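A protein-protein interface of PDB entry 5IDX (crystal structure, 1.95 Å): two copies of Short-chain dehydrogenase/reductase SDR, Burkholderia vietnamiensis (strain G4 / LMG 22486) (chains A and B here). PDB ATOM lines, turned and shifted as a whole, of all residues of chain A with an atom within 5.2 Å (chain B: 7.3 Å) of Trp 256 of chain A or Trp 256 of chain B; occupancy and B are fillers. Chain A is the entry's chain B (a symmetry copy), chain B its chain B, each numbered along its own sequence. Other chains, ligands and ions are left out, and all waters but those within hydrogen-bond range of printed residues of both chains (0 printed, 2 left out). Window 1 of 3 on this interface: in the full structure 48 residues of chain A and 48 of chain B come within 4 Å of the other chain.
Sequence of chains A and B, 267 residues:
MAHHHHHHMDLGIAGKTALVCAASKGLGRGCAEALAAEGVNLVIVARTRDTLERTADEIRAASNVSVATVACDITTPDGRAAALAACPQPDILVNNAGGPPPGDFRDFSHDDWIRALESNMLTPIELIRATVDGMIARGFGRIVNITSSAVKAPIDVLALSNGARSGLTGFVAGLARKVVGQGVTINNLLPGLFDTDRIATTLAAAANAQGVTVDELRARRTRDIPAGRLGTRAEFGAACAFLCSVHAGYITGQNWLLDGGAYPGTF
Ala 239 of chain A touches Phe 242 of chain B, and with the chains exchanged Phe 242 of chain A touches Ala 239 of chain B. Ile 251 of chain A touches Leu 258 of chain B, and with the chains exchanged Leu 258 of chain A touches Ile 251 of chain B. Gln 254 of chain A touches Leu 257 of chain B, and with the chains exchanged Leu 257 of chain A touches Gln 254 of chain B. Trp 256 of chain B touches its own counterpart, Trp 256 of chain A. Positions printed for both chains: 188, 189, 190, 239, 242, 243, 251, 254, 255, 256, 257 and 258. Of the 8 pairs that touch across the chains among the printed residues, 7 have their exchanged pair printed and touching as well.
Of chain B, only Trp 256 comes within 4 Å of Trp 256 of chain A. Trp 256 of chain B touches just one residue of chain A: Trp 256 (3.3 Å). Printed residues of chain A within 4 Å of Gln 254 of chain B: Leu 257. Of the printed residues of chain B, Gln 254 of chain A touches Leu 257 (3.4 Å). Lys 152 of chain B touches none of the printed residues of chain A. Asn 187 of chain B touches none of the printed residues of chain A. The nearest residue of chain B that does not touch Trp 256 of chain A is Gln 254 of chain B (5.1 Å). The nearest printed residue of chain A that does not touch Ala 239 of chain B is Ile 251 of chain A (4.9 Å).
NE1 of Trp 256 of chain A lies close to NE1 of Trp 256 of chain B, at 3.4 Å.
Among the printed residues, merely in contact across the chains: Ala 239 of chain A with Phe 242 of chain B (3.6 Å), Phe 242 of chain A with Ala 238 of chain B (3.7 Å), Phe 242 of chain A with Ala 239 of chain B (3.6 Å), Ile 251 of chain A with Leu 258 of chain B (3.7 Å), Gln 254 of chain A with Leu 257 of chain B (3.4 Å), Leu 257 of chain A with Gln 254 of chain B (3.4 Å) and Leu 258 of chain A with Ile 251 of chain B (3.7 Å).
Of the 12 printed residues of chain A, 7 touch a printed residue of chain B. Hydrophobic or aromatic side chains of chain A that line the printed part of chain B: Phe 242, Ile 251, Trp 256, Leu 257 and Leu 258. Of the 24 printed residues of chain B, 8 touch a printed residue of chain A. Printed residues of chain B that touch a printed residue of chain A: Ala 238, Ala 239, Phe 242, Ile 251, Gln 254, Trp 256, Leu 257 and Leu 258. Hydrophobic or aromatic side chains of chain B that line the printed part of chain A: Phe 242, Ile 251, Trp 256, Leu 257 and Leu 258. Among the printed residues, 8 pairs touch across the chains. Among the printed residues, no Asp or Glu carboxylate lies within 4 Å of a Lys or Arg side-chain nitrogen of the other chain.
The backbone carbonyl oxygen (O) of Ile 251 of chain B is in hydrogen-bond range of the side-chain amide nitrogen (ND2) of Asn 187 of chain B, at 3.0 Å. The backbone carbonyl oxygen (O) of Gln 254 of chain B sits at hydrogen-bond distance from the backbone NH (N) of Asn 188 of chain B, 2.9 Å away. The backbone carbonyl oxygen of Asn 188 of chain B is in hydrogen-bond range of the backbone NH of Trp 256 of chain B. The backbone NH (N) of Leu 190 of chain B lies within hydrogen-bond range of the backbone carbonyl oxygen (O) of Trp 256 of chain B, at 2.9 Å. N of Asn 188 of chain A is in hydrogen-bond range of O of Gln 254 of chain A, at 2.9 Å. The backbone carbonyl oxygen of Leu 190 of chain A lies within hydrogen-bond range of the backbone NH of Leu 258 of chain A (3.0 Å).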
ATOM      1  N   ASN A 188     -19.647  -2.921  28.040  1.00  0.00           N
ATOM      2  CA  ASN A 188     -18.396  -3.265  27.384  1.00  0.00           C
ATOM      3  C   ASN A 188     -17.584  -2.002  27.150  1.00  0.00           C
ATOM      4  O   ASN A 188     -18.130  -0.971  26.739  1.00  0.00           O
ATOM      5  CB  ASN A 188     -18.663  -3.991  26.055  1.00  0.00           C
ATOM      6  CG  ASN A 188     -19.613  -5.155  26.222  1.00  0.00           C
ATOM      7  OD1 ASN A 188     -19.468  -5.953  27.156  1.00  0.00           O
ATOM      8  ND2 ASN A 188     -20.614  -5.252  25.336  1.00  0.00           N
ATOM      9  N   LEU A 189     -16.284  -2.084  27.432  1.00  0.00           N
ATOM     10  CA  LEU A 189     -15.331  -1.034  27.103  1.00  0.00           C
ATOM     11  C   LEU A 189     -14.500  -1.487  25.914  1.00  0.00           C
ATOM     12  O   LEU A 189     -13.954  -2.597  25.924  1.00  0.00           O
ATOM     13  CB  LEU A 189     -14.428  -0.711  28.298  1.00  0.00           C
ATOM     14  CG  LEU A 189     -15.005   0.177  29.403  1.00  0.00           C
ATOM     15  CD1 LEU A 189     -13.955   0.390  30.496  1.00  0.00           C
ATOM     16  CD2 LEU A 189     -15.455   1.524  28.838  1.00  0.00           C
ATOM     17  N   LEU A 190     -14.423  -0.637  24.884  1.00  0.00           N
ATOM     18  CA  LEU A 190     -13.817  -0.976  23.597  1.00  0.00           C
ATOM     19  C   LEU A 190     -12.559  -0.143  23.376  1.00  0.00           C
ATOM     20  O   LEU A 190     -12.625   0.960  22.803  1.00  0.00           O
ATOM     21  CB  LEU A 190     -14.816  -0.752  22.451  1.00  0.00           C
ATOM     22  CG  LEU A 190     -15.934  -1.788  22.249  1.00  0.00           C
ATOM     23  CD1 LEU A 190     -16.881  -1.859  23.473  1.00  0.00           C
ATOM     24  CD2 LEU A 190     -16.720  -1.460  20.996  1.00  0.00           C
ATOM     25  N   ALA A 239     -12.778   5.277  33.251  1.00  0.00           N
ATOM     26  CA  ALA A 239     -14.064   4.960  32.648  1.00  0.00           C
ATOM     27  C   ALA A 239     -14.642   3.684  33.239  1.00  0.00           C
ATOM     28  O   ALA A 239     -15.846   3.604  33.509  1.00  0.00           O
ATOM     29  CB  ALA A 239     -13.921   4.833  31.128  1.00  0.00           C
ATOM     30  N   PHE A 242     -16.122   4.577  36.628  1.00  0.00           N
ATOM     31  CA  PHE A 242     -17.411   5.253  36.515  1.00  0.00           C
ATOM     32  C   PHE A 242     -18.534   4.266  36.199  1.00  0.00           C
ATOM     33  O   PHE A 242     -19.627   4.342  36.780  1.00  0.00           O
ATOM     34  CB  PHE A 242     -17.372   6.346  35.449  1.00  0.00           C
ATOM     35  CG  PHE A 242     -18.641   7.106  35.381  1.00  0.00           C
ATOM     36  CD1 PHE A 242     -18.891   8.116  36.293  1.00  0.00           C
ATOM     37  CD2 PHE A 242     -19.633   6.750  34.477  1.00  0.00           C
ATOM     38  CE1 PHE A 242     -20.100   8.815  36.263  1.00  0.00           C
ATOM     39  CE2 PHE A 242     -20.835   7.430  34.446  1.00  0.00           C
ATOM     40  CZ  PHE A 242     -21.065   8.467  35.345  1.00  0.00           C
ATOM     41  N   LEU A 243     -18.299   3.348  35.266  1.00  0.00           N
ATOM     42  CA  LEU A 243     -19.327   2.353  34.965  1.00  0.00           C
ATOM     43  C   LEU A 243     -19.657   1.502  36.183  1.00  0.00           C
ATOM     44  O   LEU A 243     -20.801   1.056  36.338  1.00  0.00           O
ATOM     45  CB  LEU A 243     -18.884   1.458  33.806  1.00  0.00           C
ATOM     46  CG  LEU A 243     -19.028   2.009  32.385  1.00  0.00           C
ATOM     47  CD1 LEU A 243     -18.385   1.028  31.392  1.00  0.00           C
ATOM     48  CD2 LEU A 243     -20.497   2.257  32.049  1.00  0.00           C
ATOM     49  N   ILE A 251     -27.268   2.692  33.092  1.00  0.00           N
ATOM     50  CA  ILE A 251     -26.466   2.463  31.897  1.00  0.00           C
ATOM     51  C   ILE A 251     -26.192   0.970  31.814  1.00  0.00           C
ATOM     52  O   ILE A 251     -25.521   0.412  32.687  1.00  0.00           O
ATOM     53  CB  ILE A 251     -25.154   3.257  31.944  1.00  0.00           C
ATOM     54  CG1 ILE A 251     -25.440   4.754  32.081  1.00  0.00           C
ATOM     55  CG2 ILE A 251     -24.301   2.958  30.708  1.00  0.00           C
ATOM     56  CD1 ILE A 251     -24.166   5.590  32.246  1.00  0.00           C
ATOM     57  N   GLN A 254     -24.147  -1.156  27.083  1.00  0.00           N
ATOM     58  CA  GLN A 254     -23.525  -0.161  26.227  1.00  0.00           C
ATOM     59  C   GLN A 254     -22.143  -0.632  25.775  1.00  0.00           C
ATOM     60  O   GLN A 254     -21.535  -1.526  26.371  1.00  0.00           O
ATOM     61  CB  GLN A 254     -23.457   1.185  26.956  1.00  0.00           C
ATOM     62  CG  GLN A 254     -24.865   1.753  27.265  1.00  0.00           C
ATOM     63  CD  GLN A 254     -25.785   1.734  26.037  1.00  0.00           C
ATOM     64  OE1 GLN A 254     -25.523   2.419  25.050  1.00  0.00           O
ATOM     65  NE2 GLN A 254     -26.860   0.938  26.095  1.00  0.00           N
ATOM     66  N   ASN A 255     -21.665  -0.041  24.677  1.00  0.00           N
ATOM     67  CA  ASN A 255     -20.350  -0.346  24.105  1.00  0.00           C
ATOM     68  C   ASN A 255     -19.624   0.987  23.963  1.00  0.00           C
ATOM     69  O   ASN A 255     -19.782   1.678  22.953  1.00  0.00           O
ATOM     70  CB  ASN A 255     -20.478  -1.074  22.762  1.00  0.00           C
ATOM     71  CG  ASN A 255     -20.988  -2.488  22.921  1.00  0.00           C
ATOM     72  OD1 ASN A 255     -20.216  -3.417  23.167  1.00  0.00           O
ATOM     73  ND2 ASN A 255     -22.298  -2.660  22.791  1.00  0.00           N
ATOM     74  N   TRP A 256     -18.851   1.342  24.984  1.00  0.00           N
ATOM     75  CA  TRP A 256     -18.180   2.632  25.047  1.00  0.00           C
ATOM     76  C   TRP A 256     -16.845   2.541  24.330  1.00  0.00           C
ATOM     77  O   TRP A 256     -15.969   1.770  24.730  1.00  0.00           O
ATOM     78  CB  TRP A 256     -17.988   3.067  26.494  1.00  0.00           C
ATOM     79  CG  TRP A 256     -19.229   3.644  27.072  1.00  0.00           C
ATOM     80  CD1 TRP A 256     -20.458   3.699  26.479  1.00  0.00           C
ATOM     81  CD2 TRP A 256     -19.366   4.273  28.351  1.00  0.00           C
ATOM     82  NE1 TRP A 256     -21.356   4.317  27.318  1.00  0.00           N
ATOM     83  CE2 TRP A 256     -20.711   4.678  28.473  1.00  0.00           C
ATOM     84  CE3 TRP A 256     -18.487   4.514  29.412  1.00  0.00           C
ATOM     85  CZ2 TRP A 256     -21.196   5.317  29.609  1.00  0.00           C
ATOM     86  CZ3 TRP A 256     -18.967   5.159  30.532  1.00  0.00           C
ATOM     87  CH2 TRP A 256     -20.311   5.553  30.621  1.00  0.00           C
ATOM     88  N   LEU A 257     -16.694   3.343  23.285  1.00  0.00           N
ATOM     89  CA  LEU A 257     -15.501   3.337  22.453  1.00  0.00           C
ATOM     90  C   LEU A 257     -14.499   4.345  23.008  1.00  0.00           C
ATOM     91  O   LEU A 257     -14.801   5.539  23.101  1.00  0.00           O
ATOM     92  CB  LEU A 257     -15.892   3.685  21.017  1.00  0.00           C
ATOM     93  CG  LEU A 257     -14.912   3.482  19.883  1.00  0.00           C
ATOM     94  CD1 LEU A 257     -14.446   2.060  19.884  1.00  0.00           C
ATOM     95  CD2 LEU A 257     -15.610   3.807  18.568  1.00  0.00           C
ATOM     96  N   LEU A 258     -13.313   3.868  23.372  1.00  0.00           N
ATOM     97  CA  LEU A 258     -12.226   4.715  23.864  1.00  0.00           C
ATOM     98  C   LEU A 258     -11.083   4.577  22.870  1.00  0.00           C
ATOM     99  O   LEU A 258     -10.170   3.766  23.056  1.00  0.00           O
ATOM    100  CB  LEU A 258     -11.793   4.312  25.285  1.00  0.00           C
ATOM    101  CG  LEU A 258     -12.595   4.923  26.440  1.00  0.00           C
ATOM    102  CD1 LEU A 258     -14.032   4.457  26.412  1.00  0.00           C
ATOM    103  CD2 LEU A 258     -11.952   4.577  27.784  1.00  0.00           C
ATOM    104  N   THR B 147     -29.232  15.177  23.837  1.00  0.00           N
ATOM    105  CA  THR B 147     -30.177  14.914  22.754  1.00  0.00           C
ATOM    106  C   THR B 147     -31.297  14.034  23.285  1.00  0.00           C
ATOM    107  O   THR B 147     -32.049  14.478  24.161  1.00  0.00           O
ATOM    108  CB  THR B 147     -29.472  14.303  21.532  1.00  0.00           C
ATOM    109  OG1 THR B 147     -28.844  13.065  21.895  1.00  0.00           O
ATOM    110  CG2 THR B 147     -28.405  15.273  21.014  1.00  0.00           C
ATOM    111  N   SER B 148     -31.404  12.789  22.812  1.00  0.00           N
ATOM    112  CA  SER B 148     -32.514  11.935  23.222  1.00  0.00           C
ATOM    113  C   SER B 148     -32.249  10.496  22.809  1.00  0.00           C
ATOM    114  O   SER B 148     -31.640  10.243  21.766  1.00  0.00           O
ATOM    115  CB  SER B 148     -33.837  12.382  22.594  1.00  0.00           C
ATOM    116  OG  SER B 148     -34.867  11.494  23.010  1.00  0.00           O
ATOM    117  N   SER B 149     -32.749   9.559  23.615  1.00  0.00           N
ATOM    118  CA  SER B 149     -32.739   8.164  23.185  1.00  0.00           C
ATOM    119  C   SER B 149     -33.510   7.974  21.884  1.00  0.00           C
ATOM    120  O   SER B 149     -33.271   6.991  21.174  1.00  0.00           O
ATOM    121  CB  SER B 149     -33.299   7.252  24.286  1.00  0.00           C
ATOM    122  OG  SER B 149     -34.670   7.485  24.529  1.00  0.00           O
ATOM    123  N   LYS B 152     -31.659   7.026  18.711  1.00  0.00           N
ATOM    124  CA  LYS B 152     -31.394   5.624  18.402  1.00  0.00           C
ATOM    125  C   LYS B 152     -32.625   4.912  17.876  1.00  0.00           C
ATOM    126  O   LYS B 152     -32.497   3.997  17.058  1.00  0.00           O
ATOM    127  CB  LYS B 152     -30.899   4.875  19.642  1.00  0.00           C
ATOM    128  CG  LYS B 152     -29.689   5.485  20.327  1.00  0.00           C
ATOM    129  CD  LYS B 152     -28.439   5.377  19.481  1.00  0.00           C
ATOM    130  CE  LYS B 152     -27.946   3.953  19.395  1.00  0.00           C
ATOM    131  NZ  LYS B 152     -26.601   3.917  18.766  1.00  0.00           N
ATOM    132  N   ASN B 187     -19.361  15.196  22.582  1.00  0.00           N
ATOM    133  CA  ASN B 187     -20.075  13.958  22.836  1.00  0.00           C
ATOM    134  C   ASN B 187     -21.543  14.268  23.090  1.00  0.00           C
ATOM    135  O   ASN B 187     -21.906  15.372  23.503  1.00  0.00           O
ATOM    136  CB  ASN B 187     -19.487  13.211  24.037  1.00  0.00           C
ATOM    137  CG  ASN B 187     -18.087  12.704  23.775  1.00  0.00           C
ATOM    138  OD1 ASN B 187     -17.891  11.786  22.971  1.00  0.00           O
ATOM    139  ND2 ASN B 187     -17.103  13.282  24.466  1.00  0.00           N
ATOM    140  N   ASN B 188     -22.387  13.278  22.860  1.00  0.00           N
ATOM    141  CA  ASN B 188     -23.821  13.438  23.036  1.00  0.00           C
ATOM    142  C   ASN B 188     -24.301  12.509  24.139  1.00  0.00           C
ATOM    143  O   ASN B 188     -23.887  11.345  24.204  1.00  0.00           O
ATOM    144  CB  ASN B 188     -24.564  13.148  21.721  1.00  0.00           C
ATOM    145  CG  ASN B 188     -23.994  13.930  20.560  1.00  0.00           C
ATOM    146  OD1 ASN B 188     -23.736  15.133  20.682  1.00  0.00           O
ATOM    147  ND2 ASN B 188     -23.764  13.250  19.427  1.00  0.00           N
ATOM    148  N   LEU B 189     -25.161  13.035  25.012  1.00  0.00           N
ATOM    149  CA  LEU B 189     -25.854  12.246  26.018  1.00  0.00           C
ATOM    150  C   LEU B 189     -27.303  12.077  25.591  1.00  0.00           C
ATOM    151  O   LEU B 189     -27.972  13.064  25.260  1.00  0.00           O
ATOM    152  CB  LEU B 189     -25.775  12.912  27.396  1.00  0.00           C
ATOM    153  CG  LEU B 189     -24.473  12.751  28.187  1.00  0.00           C
ATOM    154  CD1 LEU B 189     -24.593  13.475  29.530  1.00  0.00           C
ATOM    155  CD2 LEU B 189     -24.153  11.274  28.413  1.00  0.00           C
ATOM    156  N   LEU B 190     -27.778  10.827  25.580  1.00  0.00           N
ATOM    157  CA  LEU B 190     -29.084  10.461  25.033  1.00  0.00           C
ATOM    158  C   LEU B 190     -30.000   9.973  26.150  1.00  0.00           C
ATOM    159  O   LEU B 190     -30.037   8.766  26.454  1.00  0.00           O
ATOM    160  CB  LEU B 190     -28.937   9.381  23.951  1.00  0.00           C
ATOM    161  CG  LEU B 190     -28.425   9.806  22.564  1.00  0.00           C
ATOM    162  CD1 LEU B 190     -26.985  10.373  22.632  1.00  0.00           C
ATOM    163  CD2 LEU B 190     -28.483   8.630  21.611  1.00  0.00           C
ATOM    164  N   PRO B 191     -30.781  10.850  26.779  1.00  0.00           N
ATOM    165  CA  PRO B 191     -31.630  10.403  27.889  1.00  0.00           C
ATOM    166  C   PRO B 191     -32.838   9.618  27.404  1.00  0.00           C
ATOM    167  O   PRO B 191     -33.478   9.970  26.410  1.00  0.00           O
ATOM    168  CB  PRO B 191     -32.064  11.718  28.552  1.00  0.00           C
ATOM    169  CG  PRO B 191     -32.003  12.730  27.427  1.00  0.00           C
ATOM    170  CD  PRO B 191     -30.815  12.316  26.604  1.00  0.00           C
ATOM    171  N   PHE B 236     -27.612  11.593  35.579  1.00  0.00           N
ATOM    172  CA  PHE B 236     -27.357  12.186  34.275  1.00  0.00           C
ATOM    173  C   PHE B 236     -26.248  13.227  34.374  1.00  0.00           C
ATOM    174  O   PHE B 236     -25.297  13.220  33.581  1.00  0.00           O
ATOM    175  CB  PHE B 236     -28.638  12.804  33.723  1.00  0.00           C
ATOM    176  CG  PHE B 236     -28.517  13.261  32.289  1.00  0.00           C
ATOM    177  CD1 PHE B 236     -28.794  12.388  31.248  1.00  0.00           C
ATOM    178  CD2 PHE B 236     -28.112  14.558  31.986  1.00  0.00           C
ATOM    179  CE1 PHE B 236     -28.683  12.804  29.915  1.00  0.00           C
ATOM    180  CE2 PHE B 236     -27.981  14.976  30.664  1.00  0.00           C
ATOM    181  CZ  PHE B 236     -28.277  14.099  29.625  1.00  0.00           C
ATOM    182  N   ALA B 238     -23.942  13.305  36.555  1.00  0.00           N
ATOM    183  CA  ALA B 238     -22.675  12.634  36.845  1.00  0.00           C
ATOM    184  C   ALA B 238     -21.993  12.165  35.569  1.00  0.00           C
ATOM    185  O   ALA B 238     -20.772  12.307  35.417  1.00  0.00           O
ATOM    186  CB  ALA B 238     -22.892  11.459  37.808  1.00  0.00           C
ATOM    187  N   ALA B 239     -22.768  11.609  34.633  1.00  0.00           N
ATOM    188  CA  ALA B 239     -22.200  11.203  33.356  1.00  0.00           C
ATOM    189  C   ALA B 239     -21.693  12.408  32.579  1.00  0.00           C
ATOM    190  O   ALA B 239     -20.619  12.357  31.968  1.00  0.00           O
ATOM    191  CB  ALA B 239     -23.237  10.430  32.536  1.00  0.00           C
ATOM    192  N   CYS B 240     -22.453  13.505  32.596  1.00  0.00           N
ATOM    193  CA  CYS B 240     -21.983  14.739  31.978  1.00  0.00           C
ATOM    194  C   CYS B 240     -20.638  15.162  32.555  1.00  0.00           C
ATOM    195  O   CYS B 240     -19.704  15.472  31.810  1.00  0.00           O
ATOM    196  CB  CYS B 240     -23.017  15.852  32.177  1.00  0.00           C
ATOM    197  SG  CYS B 240     -22.607  17.384  31.317  1.00  0.00           S
ATOM    198  N   PHE B 242     -18.342  13.397  34.087  1.00  0.00           N
ATOM    199  CA  PHE B 242     -17.258  12.515  33.665  1.00  0.00           C
ATOM    200  C   PHE B 242     -16.799  12.835  32.243  1.00  0.00           C
ATOM    201  O   PHE B 242     -15.593  12.872  31.960  1.00  0.00           O
ATOM    202  CB  PHE B 242     -17.670  11.048  33.755  1.00  0.00           C
ATOM    203  CG  PHE B 242     -16.555  10.133  33.421  1.00  0.00           C
ATOM    204  CD1 PHE B 242     -15.593   9.838  34.372  1.00  0.00           C
ATOM    205  CD2 PHE B 242     -16.401   9.645  32.130  1.00  0.00           C
ATOM    206  CE1 PHE B 242     -14.516   9.007  34.056  1.00  0.00           C
ATOM    207  CE2 PHE B 242     -15.334   8.829  31.807  1.00  0.00           C
ATOM    208  CZ  PHE B 242     -14.389   8.511  32.778  1.00  0.00           C
ATOM    209  N   LEU B 243     -17.740  13.042  31.327  1.00  0.00           N
ATOM    210  CA  LEU B 243     -17.348  13.396  29.964  1.00  0.00           C
ATOM    211  C   LEU B 243     -16.566  14.702  29.928  1.00  0.00           C
ATOM    212  O   LEU B 243     -15.690  14.879  29.072  1.00  0.00           O
ATOM    213  CB  LEU B 243     -18.579  13.499  29.061  1.00  0.00           C
ATOM    214  CG  LEU B 243     -19.182  12.197  28.527  1.00  0.00           C
ATOM    215  CD1 LEU B 243     -20.488  12.510  27.783  1.00  0.00           C
ATOM    216  CD2 LEU B 243     -18.186  11.472  27.624  1.00  0.00           C
ATOM    217  N   ALA B 248     -11.498  11.965  30.212  1.00  0.00           N
ATOM    218  CA  ALA B 248     -12.312  11.604  29.057  1.00  0.00           C
ATOM    219  C   ALA B 248     -11.791  12.210  27.756  1.00  0.00           C
ATOM    220  O   ALA B 248     -12.552  12.331  26.793  1.00  0.00           O
ATOM    221  CB  ALA B 248     -13.767  12.011  29.290  1.00  0.00           C
ATOM    222  N   ILE B 251     -12.227  10.220  24.453  1.00  0.00           N
ATOM    223  CA  ILE B 251     -13.606   9.869  24.138  1.00  0.00           C
ATOM    224  C   ILE B 251     -14.207  11.033  23.368  1.00  0.00           C
ATOM    225  O   ILE B 251     -14.337  12.135  23.909  1.00  0.00           O
ATOM    226  CB  ILE B 251     -14.415   9.581  25.410  1.00  0.00           C
ATOM    227  CG1 ILE B 251     -13.772   8.443  26.206  1.00  0.00           C
ATOM    228  CG2 ILE B 251     -15.873   9.271  25.062  1.00  0.00           C
ATOM    229  CD1 ILE B 251     -14.472   8.184  27.545  1.00  0.00           C
ATOM    230  N   GLY B 253     -17.098  12.100  19.906  1.00  0.00           N
ATOM    231  CA  GLY B 253     -18.080  11.649  18.940  1.00  0.00           C
ATOM    232  C   GLY B 253     -18.941  10.506  19.424  1.00  0.00           C
ATOM    233  O   GLY B 253     -19.508   9.776  18.610  1.00  0.00           O
ATOM    234  N   GLN B 254     -19.067  10.327  20.729  1.00  0.00           N
ATOM    235  CA  GLN B 254     -19.828   9.191  21.220  1.00  0.00           C
ATOM    236  C   GLN B 254     -21.272   9.600  21.509  1.00  0.00           C
ATOM    237  O   GLN B 254     -21.594  10.782  21.663  1.00  0.00           O
ATOM    238  CB  GLN B 254     -19.145   8.601  22.458  1.00  0.00           C
ATOM    239  CG  GLN B 254     -17.744   8.027  22.133  1.00  0.00           C
ATOM    240  CD  GLN B 254     -17.760   7.103  20.907  1.00  0.00           C
ATOM    241  OE1 GLN B 254     -18.391   6.048  20.931  1.00  0.00           O
ATOM    242  NE2 GLN B 254     -17.074   7.508  19.832  1.00  0.00           N
ATOM    243  N   ASN B 255     -22.157   8.600  21.543  1.00  0.00           N
ATOM    244  CA  ASN B 255     -23.582   8.794  21.826  1.00  0.00           C
ATOM    245  C   ASN B 255     -23.926   7.846  22.970  1.00  0.00           C
ATOM    246  O   ASN B 255     -24.243   6.676  22.736  1.00  0.00           O
ATOM    247  CB  ASN B 255     -24.441   8.528  20.585  1.00  0.00           C
ATOM    248  CG  ASN B 255     -24.274   9.598  19.530  1.00  0.00           C
ATOM    249  OD1 ASN B 255     -24.937  10.636  19.569  1.00  0.00           O
ATOM    250  ND2 ASN B 255     -23.375   9.357  18.584  1.00  0.00           N
ATOM    251  N   TRP B 256     -23.840   8.354  24.195  1.00  0.00           N
ATOM    252  CA  TRP B 256     -24.030   7.548  25.391  1.00  0.00           C
ATOM    253  C   TRP B 256     -25.508   7.496  25.736  1.00  0.00           C
ATOM    254  O   TRP B 256     -26.126   8.527  26.013  1.00  0.00           O
ATOM    255  CB  TRP B 256     -23.225   8.116  26.555  1.00  0.00           C
ATOM    256  CG  TRP B 256     -21.792   7.733  26.480  1.00  0.00           C
ATOM    257  CD1 TRP B 256     -21.178   7.059  25.463  1.00  0.00           C
ATOM    258  CD2 TRP B 256     -20.788   7.976  27.471  1.00  0.00           C
ATOM    259  NE1 TRP B 256     -19.847   6.877  25.758  1.00  0.00           N
ATOM    260  CE2 TRP B 256     -19.583   7.431  26.984  1.00  0.00           C
ATOM    261  CE3 TRP B 256     -20.787   8.620  28.712  1.00  0.00           C
ATOM    262  CZ2 TRP B 256     -18.391   7.503  27.697  1.00  0.00           C
ATOM    263  CZ3 TRP B 256     -19.607   8.679  29.424  1.00  0.00           C
ATOM    264  CH2 TRP B 256     -18.425   8.123  28.913  1.00  0.00           C
ATOM    265  N   LEU B 257     -26.060   6.291  25.730  1.00  0.00           N
ATOM    266  CA  LEU B 257     -27.477   6.071  25.977  1.00  0.00           C
ATOM    267  C   LEU B 257     -27.696   5.851  27.471  1.00  0.00           C
ATOM    268  O   LEU B 257     -27.136   4.916  28.052  1.00  0.00           O
ATOM    269  CB  LEU B 257     -27.943   4.861  25.168  1.00  0.00           C
ATOM    270  CG  LEU B 257     -29.418   4.565  25.008  1.00  0.00           C
ATOM    271  CD1 LEU B 257     -30.100   5.769  24.439  1.00  0.00           C
ATOM    272  CD2 LEU B 257     -29.580   3.375  24.071  1.00  0.00           C
ATOM    273  N   LEU B 258     -28.508   6.704  28.087  1.00  0.00           N
ATOM    274  CA  LEU B 258     -28.867   6.590  29.501  1.00  0.00           C
ATOM    275  C   LEU B 258     -30.370   6.365  29.550  1.00  0.00           C
ATOM    276  O   LEU B 258     -31.151   7.309  29.709  1.00  0.00           O
ATOM    277  CB  LEU B 258     -28.455   7.843  30.293  1.00  0.00           C
ATOM    278  CG  LEU B 258     -27.012   7.876  30.813  1.00  0.00           C
ATOM    279  CD1 LEU B 258     -26.021   7.893  29.672  1.00  0.00           C
ATOM    280  CD2 LEU B 258     -26.795   9.087  31.721  1.00  0.00           C
ATOM    281  N   ASP B 259     -30.779   5.098  29.394  1.00  0.00           N
ATOM    282  CA  ASP B 259     -32.207   4.831  29.257  1.00  0.00           C
ATOM    283  C   ASP B 259     -32.633   3.557  29.984  1.00  0.00           C
ATOM    284  O   ASP B 259     -33.702   3.018  29.683  1.00  0.00           O
ATOM    285  CB  ASP B 259     -32.603   4.745  27.766  1.00  0.00           C
ATOM    286  CG  ASP B 259     -32.138   3.444  27.094  1.00  0.00           C
ATOM    287  OD1 ASP B 259     -31.224   2.758  27.610  1.00  0.00           O
ATOM    288  OD2 ASP B 259     -32.686   3.110  26.023  1.00  0.00           O
